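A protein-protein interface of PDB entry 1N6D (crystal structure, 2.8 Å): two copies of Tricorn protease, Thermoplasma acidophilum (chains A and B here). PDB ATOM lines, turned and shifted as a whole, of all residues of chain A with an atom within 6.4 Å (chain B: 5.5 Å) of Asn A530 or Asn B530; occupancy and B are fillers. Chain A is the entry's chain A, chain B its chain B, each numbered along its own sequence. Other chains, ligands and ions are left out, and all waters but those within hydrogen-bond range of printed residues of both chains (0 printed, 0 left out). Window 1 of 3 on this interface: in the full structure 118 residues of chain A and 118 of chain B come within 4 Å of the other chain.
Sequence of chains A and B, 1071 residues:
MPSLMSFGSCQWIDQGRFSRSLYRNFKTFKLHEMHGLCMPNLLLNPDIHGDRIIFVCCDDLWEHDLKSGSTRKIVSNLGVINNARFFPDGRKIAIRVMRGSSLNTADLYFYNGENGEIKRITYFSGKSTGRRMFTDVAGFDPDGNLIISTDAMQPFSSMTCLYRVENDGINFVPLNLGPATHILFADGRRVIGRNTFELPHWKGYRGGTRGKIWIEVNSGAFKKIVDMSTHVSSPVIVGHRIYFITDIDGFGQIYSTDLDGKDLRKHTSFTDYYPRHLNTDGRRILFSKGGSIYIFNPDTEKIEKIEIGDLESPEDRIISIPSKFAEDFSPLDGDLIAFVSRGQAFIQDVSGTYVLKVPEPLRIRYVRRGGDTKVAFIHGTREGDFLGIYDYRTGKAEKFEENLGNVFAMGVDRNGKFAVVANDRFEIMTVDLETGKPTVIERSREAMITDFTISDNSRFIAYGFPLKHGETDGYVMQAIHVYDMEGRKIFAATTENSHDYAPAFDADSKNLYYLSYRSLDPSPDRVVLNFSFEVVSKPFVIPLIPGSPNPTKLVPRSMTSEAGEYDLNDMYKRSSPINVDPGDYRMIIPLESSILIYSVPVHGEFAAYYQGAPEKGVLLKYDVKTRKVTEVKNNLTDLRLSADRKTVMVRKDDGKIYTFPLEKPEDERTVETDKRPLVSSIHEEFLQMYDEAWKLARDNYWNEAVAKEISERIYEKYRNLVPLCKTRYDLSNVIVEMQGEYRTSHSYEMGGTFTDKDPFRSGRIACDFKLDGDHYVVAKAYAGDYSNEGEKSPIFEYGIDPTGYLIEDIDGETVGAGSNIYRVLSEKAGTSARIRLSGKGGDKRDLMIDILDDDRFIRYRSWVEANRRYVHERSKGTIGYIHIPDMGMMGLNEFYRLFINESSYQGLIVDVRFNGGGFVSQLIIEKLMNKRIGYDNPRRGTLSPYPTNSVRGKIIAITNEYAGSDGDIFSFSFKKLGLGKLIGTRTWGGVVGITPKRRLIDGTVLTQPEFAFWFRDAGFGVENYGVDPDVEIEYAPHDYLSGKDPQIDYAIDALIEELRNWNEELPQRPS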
ATOM      1  N   TYR A 475     -31.774  -5.761  -6.457  1.00  0.00           N
ATOM      2  CA  TYR A 475     -31.130  -4.791  -7.314  1.00  0.00           C
ATOM      3  C   TYR A 475     -31.334  -5.122  -8.783  1.00  0.00           C
ATOM      4  O   TYR A 475     -31.633  -6.266  -9.129  1.00  0.00           O
ATOM      5  CB  TYR A 475     -29.630  -4.707  -6.987  1.00  0.00           C
ATOM      6  CG  TYR A 475     -29.356  -4.211  -5.596  1.00  0.00           C
ATOM      7  CD1 TYR A 475     -29.393  -5.082  -4.510  1.00  0.00           C
ATOM      8  CD2 TYR A 475     -29.115  -2.850  -5.352  1.00  0.00           C
ATOM      9  CE1 TYR A 475     -29.206  -4.608  -3.209  1.00  0.00           C
ATOM     10  CE2 TYR A 475     -28.927  -2.368  -4.053  1.00  0.00           C
ATOM     11  CZ  TYR A 475     -28.979  -3.249  -2.985  1.00  0.00           C
ATOM     12  OH  TYR A 475     -28.861  -2.746  -1.696  1.00  0.00           O
ATOM     13  N   SER A 523     -15.834   4.645   1.012  1.00  0.00           N
ATOM     14  CA  SER A 523     -15.520   5.947   1.547  1.00  0.00           C
ATOM     15  C   SER A 523     -16.141   5.971   2.948  1.00  0.00           C
ATOM     16  O   SER A 523     -17.281   5.577   3.159  1.00  0.00           O
ATOM     17  CB  SER A 523     -16.091   7.052   0.681  1.00  0.00           C
ATOM     18  OG  SER A 523     -15.549   7.021  -0.612  1.00  0.00           O
ATOM     19  N   PRO A 524     -15.378   6.444   3.936  1.00  0.00           N
ATOM     20  CA  PRO A 524     -15.819   6.521   5.332  1.00  0.00           C
ATOM     21  C   PRO A 524     -16.858   7.607   5.566  1.00  0.00           C
ATOM     22  O   PRO A 524     -16.838   8.635   4.899  1.00  0.00           O
ATOM     23  CB  PRO A 524     -14.515   6.788   6.069  1.00  0.00           C
ATOM     24  CG  PRO A 524     -13.803   7.665   5.129  1.00  0.00           C
ATOM     25  CD  PRO A 524     -14.014   6.975   3.795  1.00  0.00           C
ATOM     26  N   ASP A 525     -17.775   7.360   6.494  1.00  0.00           N
ATOM     27  CA  ASP A 525     -18.840   8.299   6.848  1.00  0.00           C
ATOM     28  C   ASP A 525     -18.273   9.097   8.036  1.00  0.00           C
ATOM     29  O   ASP A 525     -17.694   8.514   8.942  1.00  0.00           O
ATOM     30  CB  ASP A 525     -20.092   7.488   7.241  1.00  0.00           C
ATOM     31  CG  ASP A 525     -21.249   8.361   7.751  1.00  0.00           C
ATOM     32  OD1 ASP A 525     -22.376   8.267   7.225  1.00  0.00           O
ATOM     33  OD2 ASP A 525     -21.054   9.138   8.706  1.00  0.00           O
ATOM     34  N   ARG A 526     -18.455  10.408   8.051  1.00  0.00           N
ATOM     35  CA  ARG A 526     -17.862  11.195   9.097  1.00  0.00           C
ATOM     36  C   ARG A 526     -18.610  11.268  10.393  1.00  0.00           C
ATOM     37  O   ARG A 526     -18.108  11.785  11.374  1.00  0.00           O
ATOM     38  CB  ARG A 526     -17.544  12.601   8.538  1.00  0.00           C
ATOM     39  CG  ARG A 526     -16.756  12.592   7.191  1.00  0.00           C
ATOM     40  CD  ARG A 526     -15.398  11.873   7.341  1.00  0.00           C
ATOM     41  NE  ARG A 526     -14.530  11.893   6.164  1.00  0.00           N
ATOM     42  CZ  ARG A 526     -13.429  11.143   6.056  1.00  0.00           C
ATOM     43  NH1 ARG A 526     -12.660  11.190   4.972  1.00  0.00           N
ATOM     44  NH2 ARG A 526     -13.099  10.319   7.037  1.00  0.00           N
ATOM     45  N   VAL A 527     -19.806  10.711  10.412  1.00  0.00           N
ATOM     46  CA  VAL A 527     -20.650  10.775  11.612  1.00  0.00           C
ATOM     47  C   VAL A 527     -21.034   9.390  12.157  1.00  0.00           C
ATOM     48  O   VAL A 527     -20.812   9.063  13.331  1.00  0.00           O
ATOM     49  CB  VAL A 527     -21.961  11.548  11.303  1.00  0.00           C
ATOM     50  CG1 VAL A 527     -22.883  11.564  12.521  1.00  0.00           C
ATOM     51  CG2 VAL A 527     -21.614  12.956  10.863  1.00  0.00           C
ATOM     52  N   VAL A 528     -21.633   8.588  11.288  1.00  0.00           N
ATOM     53  CA  VAL A 528     -22.077   7.250  11.639  1.00  0.00           C
ATOM     54  C   VAL A 528     -21.123   6.178  11.157  1.00  0.00           C
ATOM     55  O   VAL A 528     -20.678   6.232  10.025  1.00  0.00           O
ATOM     56  CB  VAL A 528     -23.434   6.970  11.012  1.00  0.00           C
ATOM     57  CG1 VAL A 528     -23.969   5.649  11.531  1.00  0.00           C
ATOM     58  CG2 VAL A 528     -24.388   8.108  11.301  1.00  0.00           C
ATOM     59  N   LEU A 529     -20.814   5.203  12.014  1.00  0.00           N
ATOM     60  CA  LEU A 529     -19.909   4.113  11.634  1.00  0.00           C
ATOM     61  C   LEU A 529     -20.483   3.423  10.394  1.00  0.00           C
ATOM     62  O   LEU A 529     -21.274   2.488  10.502  1.00  0.00           O
ATOM     63  CB  LEU A 529     -19.784   3.105  12.762  1.00  0.00           C
ATOM     64  CG  LEU A 529     -19.139   1.812  12.249  1.00  0.00           C
ATOM     65  CD1 LEU A 529     -17.747   2.109  11.726  1.00  0.00           C
ATOM     66  CD2 LEU A 529     -19.087   0.754  13.368  1.00  0.00           C
ATOM     67  N   ASN A 530     -20.069   3.866   9.217  1.00  0.00           N
ATOM     68  CA  ASN A 530     -20.613   3.307   7.992  1.00  0.00           C
ATOM     69  C   ASN A 530     -19.686   3.655   6.823  1.00  0.00           C
ATOM     70  O   ASN A 530     -18.839   4.531   6.959  1.00  0.00           O
ATOM     71  CB  ASN A 530     -22.022   3.891   7.783  1.00  0.00           C
ATOM     72  CG  ASN A 530     -22.712   3.336   6.554  1.00  0.00           C
ATOM     73  OD1 ASN A 530     -22.262   3.552   5.444  1.00  0.00           O
ATOM     74  ND2 ASN A 530     -23.825   2.624   6.752  1.00  0.00           N
ATOM     75  N   PHE A 531     -19.831   2.971   5.690  1.00  0.00           N
ATOM     76  CA  PHE A 531     -19.017   3.256   4.514  1.00  0.00           C
ATOM     77  C   PHE A 531     -19.919   3.191   3.313  1.00  0.00           C
ATOM     78  O   PHE A 531     -20.864   2.394   3.269  1.00  0.00           O
ATOM     79  CB  PHE A 531     -17.881   2.265   4.356  1.00  0.00           C
ATOM     80  CG  PHE A 531     -16.934   2.277   5.508  1.00  0.00           C
ATOM     81  CD1 PHE A 531     -17.172   1.497   6.648  1.00  0.00           C
ATOM     82  CD2 PHE A 531     -15.804   3.092   5.465  1.00  0.00           C
ATOM     83  CE1 PHE A 531     -16.282   1.534   7.726  1.00  0.00           C
ATOM     84  CE2 PHE A 531     -14.914   3.142   6.521  1.00  0.00           C
ATOM     85  CZ  PHE A 531     -15.142   2.361   7.660  1.00  0.00           C
ATOM     86  N   SER A 532     -19.641   4.038   2.330  1.00  0.00           N
ATOM     87  CA  SER A 532     -20.461   4.088   1.124  1.00  0.00           C
ATOM     88  C   SER A 532     -19.647   4.160  -0.156  1.00  0.00           C
ATOM     89  O   SER A 532     -18.534   4.623  -0.131  1.00  0.00           O
ATOM     90  CB  SER A 532     -21.377   5.310   1.219  1.00  0.00           C
ATOM     91  OG  SER A 532     -21.936   5.646  -0.052  1.00  0.00           O
ATOM     92  N   LEU A 892     -33.471  10.750   7.737  1.00  0.00           N
ATOM     93  CA  LEU A 892     -32.169  10.146   7.850  1.00  0.00           C
ATOM     94  C   LEU A 892     -31.283  11.079   8.697  1.00  0.00           C
ATOM     95  O   LEU A 892     -30.566  10.603   9.556  1.00  0.00           O
ATOM     96  CB  LEU A 892     -31.607   9.958   6.446  1.00  0.00           C
ATOM     97  CG  LEU A 892     -30.919   8.652   6.159  1.00  0.00           C
ATOM     98  CD1 LEU A 892     -31.767   7.463   6.644  1.00  0.00           C
ATOM     99  CD2 LEU A 892     -30.659   8.574   4.670  1.00  0.00           C
ATOM    100  N   TYR A 896     -30.096   9.960  12.744  1.00  0.00           N
ATOM    101  CA  TYR A 896     -28.715   9.863  13.148  1.00  0.00           C
ATOM    102  C   TYR A 896     -28.251  11.011  14.033  1.00  0.00           C
ATOM    103  O   TYR A 896     -27.326  10.844  14.831  1.00  0.00           O
ATOM    104  CB  TYR A 896     -27.785   9.710  11.945  1.00  0.00           C
ATOM    105  CG  TYR A 896     -27.925   8.384  11.234  1.00  0.00           C
ATOM    106  CD1 TYR A 896     -28.501   8.315   9.974  1.00  0.00           C
ATOM    107  CD2 TYR A 896     -27.487   7.207  11.815  1.00  0.00           C
ATOM    108  CE1 TYR A 896     -28.635   7.115   9.305  1.00  0.00           C
ATOM    109  CE2 TYR A 896     -27.611   5.981  11.152  1.00  0.00           C
ATOM    110  CZ  TYR A 896     -28.186   5.938   9.903  1.00  0.00           C
ATOM    111  OH  TYR A 896     -28.321   4.732   9.247  1.00  0.00           O
ATOM    112  N   LEU A 923     -33.908   1.309   5.998  1.00  0.00           N
ATOM    113  CA  LEU A 923     -32.550   1.611   6.493  1.00  0.00           C
ATOM    114  C   LEU A 923     -32.507   1.925   7.983  1.00  0.00           C
ATOM    115  O   LEU A 923     -31.535   1.588   8.662  1.00  0.00           O
ATOM    116  CB  LEU A 923     -31.957   2.800   5.745  1.00  0.00           C
ATOM    117  CG  LEU A 923     -32.031   2.649   4.237  1.00  0.00           C
ATOM    118  CD1 LEU A 923     -31.359   3.847   3.542  1.00  0.00           C
ATOM    119  CD2 LEU A 923     -31.359   1.349   3.861  1.00  0.00           C
ATOM    120  N   GLU A 926     -33.244  -1.471   9.878  1.00  0.00           N
ATOM    121  CA  GLU A 926     -32.003  -2.262   9.824  1.00  0.00           C
ATOM    122  C   GLU A 926     -31.069  -1.843  10.954  1.00  0.00           C
ATOM    123  O   GLU A 926     -30.391  -2.679  11.546  1.00  0.00           O
ATOM    124  CB  GLU A 926     -31.331  -2.071   8.457  1.00  0.00           C
ATOM    125  CG  GLU A 926     -29.940  -2.641   8.331  1.00  0.00           C
ATOM    126  CD  GLU A 926     -29.352  -2.342   6.969  1.00  0.00           C
ATOM    127  OE1 GLU A 926     -29.540  -1.215   6.461  1.00  0.00           O
ATOM    128  OE2 GLU A 926     -28.700  -3.226   6.388  1.00  0.00           O
ATOM    129  N   LYS A 927     -31.048  -0.548  11.255  1.00  0.00           N
ATOM    130  CA  LYS A 927     -30.217  -0.053  12.343  1.00  0.00           C
ATOM    131  C   LYS A 927     -30.736  -0.586  13.689  1.00  0.00           C
ATOM    132  O   LYS A 927     -30.034  -1.321  14.382  1.00  0.00           O
ATOM    133  CB  LYS A 927     -30.204   1.475  12.363  1.00  0.00           C
ATOM    134  CG  LYS A 927     -28.807   2.049  12.173  1.00  0.00           C
ATOM    135  CD  LYS A 927     -28.316   1.744  10.777  1.00  0.00           C
ATOM    136  CE  LYS A 927     -26.866   2.111  10.609  1.00  0.00           C
ATOM    137  NZ  LYS A 927     -26.425   1.803   9.216  1.00  0.00           N
ATOM    138  N   ASN A 949     -23.691   0.320  16.173  1.00  0.00           N
ATOM    139  CA  ASN A 949     -25.006   0.837  15.901  1.00  0.00           C
ATOM    140  C   ASN A 949     -26.083  -0.043  16.512  1.00  0.00           C
ATOM    141  O   ASN A 949     -27.128  -0.269  15.916  1.00  0.00           O
ATOM    142  CB  ASN A 949     -25.221   0.939  14.400  1.00  0.00           C
ATOM    143  CG  ASN A 949     -24.288   1.920  13.758  1.00  0.00           C
ATOM    144  OD1 ASN A 949     -23.240   1.555  13.238  1.00  0.00           O
ATOM    145  ND2 ASN A 949     -24.649   3.185  13.813  1.00  0.00           N
ATOM    146  N   SER B 523     -25.507  11.586   1.439  1.00  0.00           N
ATOM    147  CA  SER B 523     -25.037  11.391   0.078  1.00  0.00           C
ATOM    148  C   SER B 523     -25.403   9.946  -0.304  1.00  0.00           C
ATOM    149  O   SER B 523     -25.188   8.997   0.457  1.00  0.00           O
ATOM    150  CB  SER B 523     -23.547  11.598  -0.017  1.00  0.00           C
ATOM    151  OG  SER B 523     -23.194  12.916   0.323  1.00  0.00           O
ATOM    152  N   PRO B 524     -25.960   9.765  -1.509  1.00  0.00           N
ATOM    153  CA  PRO B 524     -26.377   8.456  -2.019  1.00  0.00           C
ATOM    154  C   PRO B 524     -25.195   7.564  -2.396  1.00  0.00           C
ATOM    155  O   PRO B 524     -24.156   8.047  -2.843  1.00  0.00           O
ATOM    156  CB  PRO B 524     -27.233   8.826  -3.231  1.00  0.00           C
ATOM    157  CG  PRO B 524     -26.550  10.006  -3.761  1.00  0.00           C
ATOM    158  CD  PRO B 524     -26.270  10.818  -2.492  1.00  0.00           C
ATOM    159  N   ASP B 525     -25.351   6.265  -2.187  1.00  0.00           N
ATOM    160  CA  ASP B 525     -24.337   5.268  -2.521  1.00  0.00           C
ATOM    161  C   ASP B 525     -24.663   4.817  -3.962  1.00  0.00           C
ATOM    162  O   ASP B 525     -25.813   4.553  -4.296  1.00  0.00           O
ATOM    163  CB  ASP B 525     -24.454   4.114  -1.509  1.00  0.00           C
ATOM    164  CG  ASP B 525     -23.503   2.950  -1.795  1.00  0.00           C
ATOM    165  OD1 ASP B 525     -22.714   2.550  -0.908  1.00  0.00           O
ATOM    166  OD2 ASP B 525     -23.550   2.399  -2.910  1.00  0.00           O
ATOM    167  N   VAL B 528     -24.895   0.122  -3.480  1.00  0.00           N
ATOM    168  CA  VAL B 528     -25.772  -0.426  -2.455  1.00  0.00           C
ATOM    169  C   VAL B 528     -26.779   0.578  -1.939  1.00  0.00           C
ATOM    170  O   VAL B 528     -26.428   1.716  -1.706  1.00  0.00           O
ATOM    171  CB  VAL B 528     -24.961  -0.907  -1.278  1.00  0.00           C
ATOM    172  CG1 VAL B 528     -25.870  -1.617  -0.303  1.00  0.00           C
ATOM    173  CG2 VAL B 528     -23.833  -1.809  -1.767  1.00  0.00           C
ATOM    174  N   LEU B 529     -28.033   0.162  -1.770  1.00  0.00           N
ATOM    175  CA  LEU B 529     -29.063   1.073  -1.276  1.00  0.00           C
ATOM    176  C   LEU B 529     -28.643   1.562   0.097  1.00  0.00           C
ATOM    177  O   LEU B 529     -28.944   0.931   1.104  1.00  0.00           O
ATOM    178  CB  LEU B 529     -30.397   0.364  -1.156  1.00  0.00           C
ATOM    179  CG  LEU B 529     -31.376   1.187  -0.300  1.00  0.00           C
ATOM    180  CD1 LEU B 529     -31.620   2.514  -0.978  1.00  0.00           C
ATOM    181  CD2 LEU B 529     -32.696   0.418  -0.102  1.00  0.00           C
ATOM    182  N   ASN B 530     -27.979   2.707   0.140  1.00  0.00           N
ATOM    183  CA  ASN B 530     -27.469   3.215   1.401  1.00  0.00           C
ATOM    184  C   ASN B 530     -27.112   4.698   1.253  1.00  0.00           C
ATOM    185  O   ASN B 530     -26.995   5.178   0.135  1.00  0.00           O
ATOM    186  CB  ASN B 530     -26.224   2.391   1.798  1.00  0.00           C
ATOM    187  CG  ASN B 530     -25.659   2.807   3.148  1.00  0.00           C
ATOM    188  OD1 ASN B 530     -25.192   3.928   3.301  1.00  0.00           O
ATOM    189  ND2 ASN B 530     -25.704   1.905   4.134  1.00  0.00           N
ATOM    190  N   PHE B 531     -26.935   5.412   2.366  1.00  0.00           N
ATOM    191  CA  PHE B 531     -26.580   6.824   2.325  1.00  0.00           C
ATOM    192  C   PHE B 531     -25.569   7.070   3.399  1.00  0.00           C
ATOM    193  O   PHE B 531     -25.605   6.439   4.466  1.00  0.00           O
ATOM    194  CB  PHE B 531     -27.782   7.725   2.541  1.00  0.00           C
ATOM    195  CG  PHE B 531     -28.839   7.553   1.502  1.00  0.00           C
ATOM    196  CD1 PHE B 531     -29.825   6.568   1.630  1.00  0.00           C
ATOM    197  CD2 PHE B 531     -28.834   8.362   0.372  1.00  0.00           C
ATOM    198  CE1 PHE B 531     -30.792   6.405   0.634  1.00  0.00           C
ATOM    199  CE2 PHE B 531     -29.784   8.212  -0.619  1.00  0.00           C
ATOM    200  CZ  PHE B 531     -30.774   7.234  -0.499  1.00  0.00           C
ATOM    201  N   SER B 532     -24.646   7.983   3.121  1.00  0.00           N
ATOM    202  CA  SER B 532     -23.584   8.282   4.082  1.00  0.00           C
ATOM    203  C   SER B 532     -23.312   9.763   4.235  1.00  0.00           C
ATOM    204  O   SER B 532     -23.571  10.520   3.328  1.00  0.00           O
ATOM    205  CB  SER B 532     -22.308   7.564   3.626  1.00  0.00           C
ATOM    206  OG  SER B 532     -21.158   8.087   4.289  1.00  0.00           O
ATOM    207  N   LEU B 923     -20.954  -4.578  10.454  1.00  0.00           N
ATOM    208  CA  LEU B 923     -21.685  -4.001   9.320  1.00  0.00           C
ATOM    209  C   LEU B 923     -22.243  -5.032   8.360  1.00  0.00           C
ATOM    210  O   LEU B 923     -23.319  -4.839   7.781  1.00  0.00           O
ATOM    211  CB  LEU B 923     -20.781  -3.063   8.527  1.00  0.00           C
ATOM    212  CG  LEU B 923     -20.112  -2.023   9.404  1.00  0.00           C
ATOM    213  CD1 LEU B 923     -19.296  -1.035   8.550  1.00  0.00           C
ATOM    214  CD2 LEU B 923     -21.196  -1.303  10.187  1.00  0.00           C
ATOM    215  N   LYS B 927     -26.356  -6.385   7.813  1.00  0.00           N
ATOM    216  CA  LYS B 927     -26.995  -6.581   6.522  1.00  0.00           C
ATOM    217  C   LYS B 927     -27.756  -7.903   6.521  1.00  0.00           C
ATOM    218  O   LYS B 927     -28.958  -7.909   6.352  1.00  0.00           O
ATOM    219  CB  LYS B 927     -25.943  -6.583   5.404  1.00  0.00           C
ATOM    220  CG  LYS B 927     -26.141  -5.487   4.380  1.00  0.00           C
ATOM    221  CD  LYS B 927     -25.934  -4.145   5.030  1.00  0.00           C
ATOM    222  CE  LYS B 927     -26.350  -3.004   4.134  1.00  0.00           C
ATOM    223  NZ  LYS B 927     -26.133  -1.693   4.829  1.00  0.00           N
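The backbone NH (N) of Leu B529 is in hydrogen-bond range of the side-chain hydroxyl (OH) of Tyr A475, 3.0 Å away.
OG of Ser B532 lies within hydrogen-bond range of OD1 of Asp A525, at 3.2 Å.
ND2 of Asn B530 lies close to ND2 of Asn A530 (3.3 Å).
The side-chain carboxylate (OD1) of Asp B525 lies close to the side-chain hydroxyl (OG) of Ser A532, 3.3 Å away.
NZ of Lys B927 is in salt-bridge range of OE2 of Glu A926 (3.4 Å).
N of Ser A523 is in hydrogen-bond range of O of Ser A532, at 2.9 Å.
The side-chain carboxylate of Asp A525 sits at hydrogen-bond distance from the backbone NH of Val A527, 2.6 Å away.
The backbone NH of Val A528 is in hydrogen-bond range of the side-chain carboxylate of Asp A525.
N of Asp A525 is in hydrogen-bond range of O of Asn A530 (3.1 Å).
The backbone carbonyl oxygen (O) of Leu A529 lies close to the side-chain amide oxygen (OD1) of Asn A949 (3.5 Å).
The backbone NH (N) of Val B528 lies within hydrogen-bond range of the side-chain carboxylate (OD2) of Asp B525 (2.7 Å).
CG1 of Val B528 touches OH of Tyr A475, 3.5 Å away.
Leu A529 touches Leu B923 (O to CD2, 3.8 Å).
Phe A531 touches Leu B923 (CD1 to CD1, 3.8 Å).
CB of Ser B532 touches CB of Ser A532, at 3.4 Å.
Leu A892 touches Phe B531.
CD2 of Leu A923 touches O of Leu B529, 3.7 Å away.
Phe B531 touches Leu A923.
Asn A530 touches just one residue of chain B: Asn B530 (3.3 Å).
Asn B530 touches just one residue of chain A: Asn A530 (3.3 Å).
Of the printed residues of chain A, Leu B529 touches Tyr A475 (3.0 Å) and Leu A923 (3.7 Å).
Of the printed residues of chain B, Leu A892 touches Phe B531 (3.7 Å).
Of the printed residues of chain B, Tyr A475 touches Val B528 (3.5 Å) and Leu B529 (3.0 Å).
Of the printed residues of chain B, Glu A926 touches Lys B927.
Of the printed residues of chain A, Ser B532 touches Asp A525 and Ser A532.
Pro B524 touches none of the printed residues of chain A.
Val A528 touches none of the printed residues of chain B.
The nearest residue of chain B that does not touch Asn A530 is Ser B532 (4.4 Å).
Hydrophobic or aromatic side chains of chain A that line the printed part of chain B: Tyr A475, Phe A531, Leu A892 and Leu A923.
Along chain A the printed residues that touch a printed residue of chain B span positions 475 to 926.
Of the 10 printed residues of chain B, 8 touch a printed residue of chain A.
Printed residues of chain B that touch a printed residue of chain A: Asp B525, Val B528, Leu B529, Asn B530, Phe B531, Ser B532, Leu B923 and Lys B927.
Hydrophobic or aromatic side chains of chain B that line the printed part of chain A: Val B528, Leu B529, Phe B531 and Leu B923.
Among the printed residues, Asp or Glu carboxylates within 4 Å of a Lys or Arg side-chain nitrogen of the other chain: Glu A926 with Lys B927.
Leu A529 touches Leu B923, and with the chains exchanged Leu A923 touches Leu B529.
Asn A530 touches its own counterpart, Asn B530.
Phe A531 touches Leu B923, and with the chains exchanged Leu A923 touches Phe B531.
Ser A532 touches its own counterpart, Ser B532.
10 positions are printed for both chains.
Of the 12 pairs that touch across the chains among the printed residues, 8 have their exchanged pair printed and touching as well.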
